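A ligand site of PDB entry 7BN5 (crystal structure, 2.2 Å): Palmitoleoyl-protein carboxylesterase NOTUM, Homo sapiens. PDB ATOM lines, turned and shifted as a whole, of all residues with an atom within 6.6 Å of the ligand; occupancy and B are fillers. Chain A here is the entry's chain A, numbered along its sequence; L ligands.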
ATOM      1  N   GLY A  49      -4.828 -30.369 -20.590  1.00  0.00           N
ATOM      2  CA  GLY A  49      -5.836 -30.088 -21.587  1.00  0.00           C
ATOM      3  C   GLY A  49      -5.231 -29.940 -22.976  1.00  0.00           C
ATOM      4  O   GLY A  49      -4.083 -30.291 -23.232  1.00  0.00           O
ATOM      5  N   GLY A  50      -6.043 -29.400 -23.882  1.00  0.00           N
ATOM      6  CA  GLY A  50      -5.584 -29.156 -25.240  1.00  0.00           C
ATOM      7  C   GLY A  50      -6.568 -29.576 -26.313  1.00  0.00           C
ATOM      8  O   GLY A  50      -6.176 -30.178 -27.317  1.00  0.00           O
ATOM      9  N   TRP A  51      -7.848 -29.250 -26.108  1.00  0.00           N
ATOM     10  CA  TRP A  51      -8.907 -29.509 -27.075  1.00  0.00           C
ATOM     11  C   TRP A  51      -9.060 -30.983 -27.412  1.00  0.00           C
ATOM     12  O   TRP A  51      -8.952 -31.831 -26.517  1.00  0.00           O
ATOM     13  CB  TRP A  51      -8.678 -28.708 -28.349  1.00  0.00           C
ATOM     14  CG  TRP A  51      -8.828 -27.251 -28.132  1.00  0.00           C
ATOM     15  CD1 TRP A  51      -7.829 -26.357 -27.879  1.00  0.00           C
ATOM     16  CD2 TRP A  51     -10.050 -26.506 -28.130  1.00  0.00           C
ATOM     17  NE1 TRP A  51      -8.360 -25.092 -27.735  1.00  0.00           N
ATOM     18  CE2 TRP A  51      -9.719 -25.162 -27.878  1.00  0.00           C
ATOM     19  CE3 TRP A  51     -11.393 -26.844 -28.318  1.00  0.00           C
ATOM     20  CZ2 TRP A  51     -10.674 -24.149 -27.814  1.00  0.00           C
ATOM     21  CZ3 TRP A  51     -12.341 -25.838 -28.255  1.00  0.00           C
ATOM     22  CH2 TRP A  51     -11.976 -24.506 -28.004  1.00  0.00           C
ATOM     23  N   TYR A  52      -9.321 -31.305 -28.674  1.00  0.00           N
ATOM     24  CA  TYR A  52      -9.655 -32.662 -29.078  1.00  0.00           C
ATOM     25  C   TYR A  52      -9.679 -32.749 -30.592  1.00  0.00           C
ATOM     26  O   TYR A  52      -9.428 -31.753 -31.296  1.00  0.00           O
ATOM     27  CB  TYR A  52     -10.999 -33.094 -28.491  1.00  0.00           C
ATOM     28  CG  TYR A  52     -12.067 -32.033 -28.663  1.00  0.00           C
ATOM     29  CD1 TYR A  52     -12.769 -31.921 -29.850  1.00  0.00           C
ATOM     30  CD2 TYR A  52     -12.361 -31.144 -27.633  1.00  0.00           C
ATOM     31  CE1 TYR A  52     -13.738 -30.950 -30.011  1.00  0.00           C
ATOM     32  CE2 TYR A  52     -13.323 -30.166 -27.793  1.00  0.00           C
ATOM     33  CZ  TYR A  52     -14.013 -30.083 -28.983  1.00  0.00           C
ATOM     34  OH  TYR A  52     -14.975 -29.106 -29.133  1.00  0.00           O
ATOM     35  N   TYR A 105      -1.466 -35.014 -22.081  1.00  0.00           N
ATOM     36  CA  TYR A 105      -2.690 -35.247 -22.843  1.00  0.00           C
ATOM     37  C   TYR A 105      -2.279 -35.649 -24.261  1.00  0.00           C
ATOM     38  O   TYR A 105      -1.902 -34.797 -25.070  1.00  0.00           O
ATOM     39  CB  TYR A 105      -3.559 -34.002 -22.829  1.00  0.00           C
ATOM     40  CG  TYR A 105      -4.878 -34.121 -23.569  1.00  0.00           C
ATOM     41  CD1 TYR A 105      -5.689 -35.227 -23.412  1.00  0.00           C
ATOM     42  CD2 TYR A 105      -5.322 -33.089 -24.393  1.00  0.00           C
ATOM     43  CE1 TYR A 105      -6.904 -35.321 -24.071  1.00  0.00           C
ATOM     44  CE2 TYR A 105      -6.529 -33.176 -25.061  1.00  0.00           C
ATOM     45  CZ  TYR A 105      -7.320 -34.292 -24.895  1.00  0.00           C
ATOM     46  OH  TYR A 105      -8.520 -34.372 -25.563  1.00  0.00           O
ATOM     47  N   VAL A 110     -10.700 -35.889 -24.707  1.00  0.00           N
ATOM     48  CA  VAL A 110     -11.168 -35.311 -23.443  1.00  0.00           C
ATOM     49  C   VAL A 110     -11.077 -36.375 -22.358  1.00  0.00           C
ATOM     50  O   VAL A 110     -11.927 -36.454 -21.462  1.00  0.00           O
ATOM     51  CB  VAL A 110     -12.595 -34.747 -23.576  1.00  0.00           C
ATOM     52  CG1 VAL A 110     -12.860 -33.724 -22.474  1.00  0.00           C
ATOM     53  CG2 VAL A 110     -12.803 -34.117 -24.942  1.00  0.00           C
ATOM     54  N   SER A 154      -6.926 -29.175 -16.258  1.00  0.00           N
ATOM     55  CA  SER A 154      -7.277 -27.882 -16.837  1.00  0.00           C
ATOM     56  C   SER A 154      -7.811 -28.065 -18.245  1.00  0.00           C
ATOM     57  O   SER A 154      -7.340 -28.941 -18.984  1.00  0.00           O
ATOM     58  CB  SER A 154      -6.072 -26.935 -16.842  1.00  0.00           C
ATOM     59  OG  SER A 154      -5.617 -26.678 -15.528  1.00  0.00           O
ATOM     60  N   SER A 155      -8.785 -27.245 -18.620  1.00  0.00           N
ATOM     61  CA  SER A 155      -9.393 -27.234 -19.959  1.00  0.00           C
ATOM     62  C   SER A 155     -10.010 -28.608 -20.201  1.00  0.00           C
ATOM     63  O   SER A 155     -10.811 -29.057 -19.370  1.00  0.00           O
ATOM     64  CB  SER A 155      -8.355 -26.791 -20.983  1.00  0.00           C
ATOM     65  OG  SER A 155      -7.996 -25.446 -20.782  1.00  0.00           O
ATOM     66  N   ALA A 156      -9.677 -29.288 -21.302  1.00  0.00           N
ATOM     67  CA  ALA A 156     -10.179 -30.645 -21.533  1.00  0.00           C
ATOM     68  C   ALA A 156      -9.750 -31.602 -20.421  1.00  0.00           C
ATOM     69  O   ALA A 156     -10.423 -32.600 -20.186  1.00  0.00           O
ATOM     70  CB  ALA A 156      -9.713 -31.150 -22.891  1.00  0.00           C
ATOM     71  N   GLY A 157      -8.643 -31.300 -19.742  1.00  0.00           N
ATOM     72  CA  GLY A 157      -8.275 -32.078 -18.573  1.00  0.00           C
ATOM     73  C   GLY A 157      -9.219 -31.859 -17.398  1.00  0.00           C
ATOM     74  O   GLY A 157      -9.447 -32.780 -16.617  1.00  0.00           O
ATOM     75  N   THR A 159     -12.511 -31.220 -17.725  1.00  0.00           N
ATOM     76  CA  THR A 159     -13.610 -32.109 -18.078  1.00  0.00           C
ATOM     77  C   THR A 159     -13.218 -33.563 -17.875  1.00  0.00           C
ATOM     78  O   THR A 159     -14.072 -34.396 -17.542  1.00  0.00           O
ATOM     79  CB  THR A 159     -14.041 -31.863 -19.527  1.00  0.00           C
ATOM     80  OG1 THR A 159     -14.211 -30.457 -19.746  1.00  0.00           O
ATOM     81  CG2 THR A 159     -15.357 -32.572 -19.820  1.00  0.00           C
ATOM     82  N   SER A 188     -11.433 -25.001 -15.501  1.00  0.00           N
ATOM     83  CA  SER A 188     -11.784 -24.530 -16.840  1.00  0.00           C
ATOM     84  C   SER A 188     -12.312 -25.660 -17.733  1.00  0.00           C
ATOM     85  O   SER A 188     -12.121 -25.638 -18.948  1.00  0.00           O
ATOM     86  CB  SER A 188     -10.595 -23.841 -17.512  1.00  0.00           C
ATOM     87  OG  SER A 188     -10.175 -22.710 -16.758  1.00  0.00           O
ATOM     88  N   GLY A 189     -12.976 -26.636 -17.134  1.00  0.00           N
ATOM     89  CA  GLY A 189     -13.576 -27.722 -17.881  1.00  0.00           C
ATOM     90  C   GLY A 189     -15.078 -27.803 -17.672  1.00  0.00           C
ATOM     91  O   GLY A 189     -15.693 -28.851 -17.893  1.00  0.00           O
ATOM     92  N   PHE A 191     -18.089 -26.517 -19.128  1.00  0.00           N
ATOM     93  CA  PHE A 191     -18.594 -25.900 -20.340  1.00  0.00           C
ATOM     94  C   PHE A 191     -20.117 -25.981 -20.422  1.00  0.00           C
ATOM     95  O   PHE A 191     -20.760 -26.826 -19.791  1.00  0.00           O
ATOM     96  CB  PHE A 191     -17.978 -26.565 -21.584  1.00  0.00           C
ATOM     97  CG  PHE A 191     -16.484 -26.455 -21.630  1.00  0.00           C
ATOM     98  CD1 PHE A 191     -15.881 -25.267 -21.998  1.00  0.00           C
ATOM     99  CD2 PHE A 191     -15.692 -27.539 -21.307  1.00  0.00           C
ATOM    100  CE1 PHE A 191     -14.501 -25.160 -22.042  1.00  0.00           C
ATOM    101  CE2 PHE A 191     -14.305 -27.440 -21.352  1.00  0.00           C
ATOM    102  CZ  PHE A 191     -13.717 -26.250 -21.720  1.00  0.00           C
ATOM    103  N   LEU A 192     -20.687 -25.082 -21.227  1.00  0.00           N
ATOM    104  CA  LEU A 192     -22.121 -25.022 -21.467  1.00  0.00           C
ATOM    105  C   LEU A 192     -22.405 -25.412 -22.896  1.00  0.00           C
ATOM    106  O   LEU A 192     -21.726 -24.950 -23.825  1.00  0.00           O
ATOM    107  CB  LEU A 192     -22.656 -23.605 -21.189  1.00  0.00           C
ATOM    108  CG  LEU A 192     -22.513 -23.057 -19.774  1.00  0.00           C
ATOM    109  CD1 LEU A 192     -23.140 -21.673 -19.659  1.00  0.00           C
ATOM    110  CD2 LEU A 192     -23.123 -24.005 -18.751  1.00  0.00           C
ATOM    111  N   PRO A 210     -20.050 -26.866 -30.659  1.00  0.00           N
ATOM    112  CA  PRO A 210     -19.453 -27.750 -29.653  1.00  0.00           C
ATOM    113  C   PRO A 210     -20.251 -29.025 -29.382  1.00  0.00           C
ATOM    114  O   PRO A 210     -19.670 -30.114 -29.318  1.00  0.00           O
ATOM    115  CB  PRO A 210     -19.381 -26.866 -28.407  1.00  0.00           C
ATOM    116  CG  PRO A 210     -20.569 -26.029 -28.507  1.00  0.00           C
ATOM    117  CD  PRO A 210     -20.832 -25.811 -29.981  1.00  0.00           C
ATOM    118  N   ILE A 214     -18.744 -33.248 -29.639  1.00  0.00           N
ATOM    119  CA  ILE A 214     -18.688 -34.295 -28.632  1.00  0.00           C
ATOM    120  C   ILE A 214     -19.527 -35.494 -29.066  1.00  0.00           C
ATOM    121  O   ILE A 214     -19.149 -36.650 -28.836  1.00  0.00           O
ATOM    122  CB  ILE A 214     -19.150 -33.748 -27.271  1.00  0.00           C
ATOM    123  CG1 ILE A 214     -18.343 -32.505 -26.893  1.00  0.00           C
ATOM    124  CG2 ILE A 214     -19.017 -34.815 -26.197  1.00  0.00           C
ATOM    125  CD1 ILE A 214     -16.852 -32.748 -26.821  1.00  0.00           C
ATOM    126  N   PHE A 242     -20.422 -34.923 -20.838  1.00  0.00           N
ATOM    127  CA  PHE A 242     -19.220 -34.116 -21.027  1.00  0.00           C
ATOM    128  C   PHE A 242     -19.402 -32.672 -20.560  1.00  0.00           C
ATOM    129  O   PHE A 242     -18.463 -31.880 -20.687  1.00  0.00           O
ATOM    130  CB  PHE A 242     -18.807 -34.106 -22.497  1.00  0.00           C
ATOM    131  CG  PHE A 242     -18.073 -35.343 -22.921  1.00  0.00           C
ATOM    132  CD1 PHE A 242     -18.715 -36.560 -22.977  1.00  0.00           C
ATOM    133  CD2 PHE A 242     -16.731 -35.276 -23.270  1.00  0.00           C
ATOM    134  CE1 PHE A 242     -18.042 -37.709 -23.362  1.00  0.00           C
ATOM    135  CE2 PHE A 242     -16.051 -36.418 -23.665  1.00  0.00           C
ATOM    136  CZ  PHE A 242     -16.706 -37.635 -23.711  1.00  0.00           C
ATOM    137  N   PHE A 243     -20.574 -32.329 -20.033  1.00  0.00           N
ATOM    138  CA  PHE A 243     -20.878 -30.967 -19.632  1.00  0.00           C
ATOM    139  C   PHE A 243     -21.108 -30.933 -18.130  1.00  0.00           C
ATOM    140  O   PHE A 243     -21.930 -31.694 -17.600  1.00  0.00           O
ATOM    141  CB  PHE A 243     -22.085 -30.430 -20.403  1.00  0.00           C
ATOM    142  CG  PHE A 243     -21.803 -30.230 -21.864  1.00  0.00           C
ATOM    143  CD1 PHE A 243     -21.976 -31.272 -22.763  1.00  0.00           C
ATOM    144  CD2 PHE A 243     -21.329 -29.021 -22.329  1.00  0.00           C
ATOM    145  CE1 PHE A 243     -21.694 -31.098 -24.105  1.00  0.00           C
ATOM    146  CE2 PHE A 243     -21.039 -28.840 -23.671  1.00  0.00           C
ATOM    147  CZ  PHE A 243     -21.232 -29.874 -24.559  1.00  0.00           C
ATOM    148  N   ASP A 263     -14.963 -18.041 -20.090  1.00  0.00           N
ATOM    149  CA  ASP A 263     -13.849 -18.870 -20.540  1.00  0.00           C
ATOM    150  C   ASP A 263     -13.588 -18.659 -22.020  1.00  0.00           C
ATOM    151  O   ASP A 263     -14.521 -18.594 -22.838  1.00  0.00           O
ATOM    152  CB  ASP A 263     -14.139 -20.339 -20.242  1.00  0.00           C
ATOM    153  CG  ASP A 263     -13.003 -21.246 -20.640  1.00  0.00           C
ATOM    154  OD1 ASP A 263     -12.026 -21.361 -19.867  1.00  0.00           O
ATOM    155  OD2 ASP A 263     -13.074 -21.844 -21.739  1.00  0.00           O
ATOM    156  N   ALA A 265     -12.136 -20.654 -24.260  1.00  0.00           N
ATOM    157  CA  ALA A 265     -12.564 -21.786 -25.084  1.00  0.00           C
ATOM    158  C   ALA A 265     -14.083 -21.819 -25.221  1.00  0.00           C
ATOM    159  O   ALA A 265     -14.605 -22.156 -26.292  1.00  0.00           O
ATOM    160  CB  ALA A 265     -12.044 -23.096 -24.488  1.00  0.00           C
ATOM    161  N   GLN A 266     -14.798 -21.478 -24.148  1.00  0.00           N
ATOM    162  CA  GLN A 266     -16.254 -21.387 -24.234  1.00  0.00           C
ATOM    163  C   GLN A 266     -16.686 -20.339 -25.257  1.00  0.00           C
ATOM    164  O   GLN A 266     -17.599 -20.584 -26.054  1.00  0.00           O
ATOM    165  CB  GLN A 266     -16.836 -21.058 -22.862  1.00  0.00           C
ATOM    166  CG  GLN A 266     -18.333 -20.815 -22.854  1.00  0.00           C
ATOM    167  CD  GLN A 266     -19.144 -22.093 -22.924  1.00  0.00           C
ATOM    168  OE1 GLN A 266     -18.905 -23.028 -22.159  1.00  0.00           O
ATOM    169  NE2 GLN A 266     -20.111 -22.137 -23.832  1.00  0.00           N
ATOM    170  N   VAL A 269     -15.921 -21.693 -29.017  1.00  0.00           N
ATOM    171  CA  VAL A 269     -16.966 -22.570 -29.559  1.00  0.00           C
ATOM    172  C   VAL A 269     -18.301 -21.867 -29.671  1.00  0.00           C
ATOM    173  O   VAL A 269     -19.216 -22.391 -30.313  1.00  0.00           O
ATOM    174  CB  VAL A 269     -17.119 -23.840 -28.692  1.00  0.00           C
ATOM    175  CG1 VAL A 269     -15.775 -24.541 -28.530  1.00  0.00           C
ATOM    176  CG2 VAL A 269     -17.723 -23.514 -27.339  1.00  0.00           C
ATOM    177  N   HIS A 312      -8.252 -18.330 -19.545  1.00  0.00           N
ATOM    178  CA  HIS A 312      -8.259 -19.764 -19.849  1.00  0.00           C
ATOM    179  C   HIS A 312      -7.240 -20.444 -18.949  1.00  0.00           C
ATOM    180  O   HIS A 312      -6.074 -20.063 -18.956  1.00  0.00           O
ATOM    181  CB  HIS A 312      -7.934 -20.009 -21.321  1.00  0.00           C
ATOM    182  CG  HIS A 312      -8.223 -21.402 -21.779  1.00  0.00           C
ATOM    183  ND1 HIS A 312      -9.456 -21.996 -21.631  1.00  0.00           N
ATOM    184  CD2 HIS A 312      -7.441 -22.319 -22.395  1.00  0.00           C
ATOM    185  CE1 HIS A 312      -9.425 -23.223 -22.127  1.00  0.00           C
ATOM    186  NE2 HIS A 312      -8.204 -23.439 -22.602  1.00  0.00           N
ATOM    187  N   GLU A 313      -7.696 -21.447 -18.193  1.00  0.00           N
ATOM    188  CA  GLU A 313      -6.870 -22.212 -17.249  1.00  0.00           C
ATOM    189  C   GLU A 313      -6.347 -21.346 -16.119  1.00  0.00           C
ATOM    190  O   GLU A 313      -6.423 -20.113 -16.185  1.00  0.00           O
ATOM    191  CB  GLU A 313      -5.705 -22.892 -17.977  1.00  0.00           C
ATOM    192  CG  GLU A 313      -6.105 -23.729 -19.165  1.00  0.00           C
ATOM    193  CD  GLU A 313      -4.965 -24.551 -19.716  1.00  0.00           C
ATOM    194  OE1 GLU A 313      -3.801 -24.153 -19.530  1.00  0.00           O
ATOM    195  OE2 GLU A 313      -5.233 -25.610 -20.334  1.00  0.00           O
HETATM  196  C1  LIG L   1     -16.823 -29.096 -24.443  1.00  0.00           C
HETATM  197  C2  LIG L   1     -15.763 -28.205 -24.692  1.00  0.00           C
HETATM  198  C3  LIG L   1     -16.014 -26.914 -25.203  1.00  0.00           C
HETATM  199  C4  LIG L   1     -14.931 -26.084 -25.438  1.00  0.00           C
HETATM  200  C5  LIG L   1     -13.434 -27.678 -24.718  1.00  0.00           C
HETATM  201  C6  LIG L   1     -10.675 -26.683 -24.695  1.00  0.00           C
HETATM  202  C7  LIG L   1      -9.244 -26.961 -24.254  1.00  0.00           C
HETATM  203  C8  LIG L   1     -14.468 -28.601 -24.452  1.00  0.00           C
HETATM  204  C9  LIG L   1     -14.196 -29.887 -23.941  1.00  0.00           C
HETATM  205  C10 LIG L   1     -15.246 -30.758 -23.690  1.00  0.00           C
HETATM  206  C11 LIG L   1     -16.564 -30.365 -23.941  1.00  0.00           C
HETATM  207  N1  LIG L   1     -13.692 -26.475 -25.196  1.00  0.00           N
HETATM  208  O1  LIG L   1      -8.900 -28.130 -23.924  1.00  0.00           O
HETATM  209  O2  LIG L   1      -8.401 -26.019 -24.205  1.00  0.00           O
HETATM  210  S1  LIG L   1     -11.704 -28.151 -24.409  1.00  0.00           S
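O of Trp 51 sits at hydrogen-bond distance from OH of Tyr 105, 2.7 Å away.
The backbone NH (N) of Ala 265 sits at hydrogen-bond distance from the side-chain carboxylate (OD2) of Asp 263 (2.9 Å).
OG of Ser 155 sits at hydrogen-bond distance from OE2 of Glu 313.
The side-chain hydroxyl of Ser 155 is in hydrogen-bond range of a ring nitrogen (NE2) of His 312, at 2.7 Å.
N of Val 110 sits at hydrogen-bond distance from OH of Tyr 105 (2.8 Å).
The side-chain carboxylate (OD1) of Asp 263 lies within hydrogen-bond range of a ring nitrogen (ND1) of His 312, 3.2 Å away.
Merely in contact with the ligand: Phe 191, Val 269, Ile 214, Ala 265, Tyr 52 and Val 110.
Hydrophobic or aromatic side chains within 4 Å of the ligand: Trp 51, Tyr 52, Val 110, Ala 156, Phe 191, Ile 214, Ala 265, Val 269 and His 312.
Of the 25 residues printed, 11 come within 4 Å of the ligand.
Along chain A the residues within 4 Å of the ligand span positions 50 to 312.
The nearest printed residue that does not touch the ligand is Phe 242 (4.1 Å).
The backbone NH (N) of Trp 51 is in hydrogen-bond range of an oxygen (O1) of the ligand.
N of Ala 156 is in hydrogen-bond range of O1 of the ligand.
An oxygen (O1) of the ligand sits at hydrogen-bond distance from the backbone NH of Gly 50 (3.1 Å).
OG of Ser 155 lies close to O2 of the ligand, at 3.5 Å.
O2 of the ligand lies within hydrogen-bond range of NE2 of His 312 (3.0 Å).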
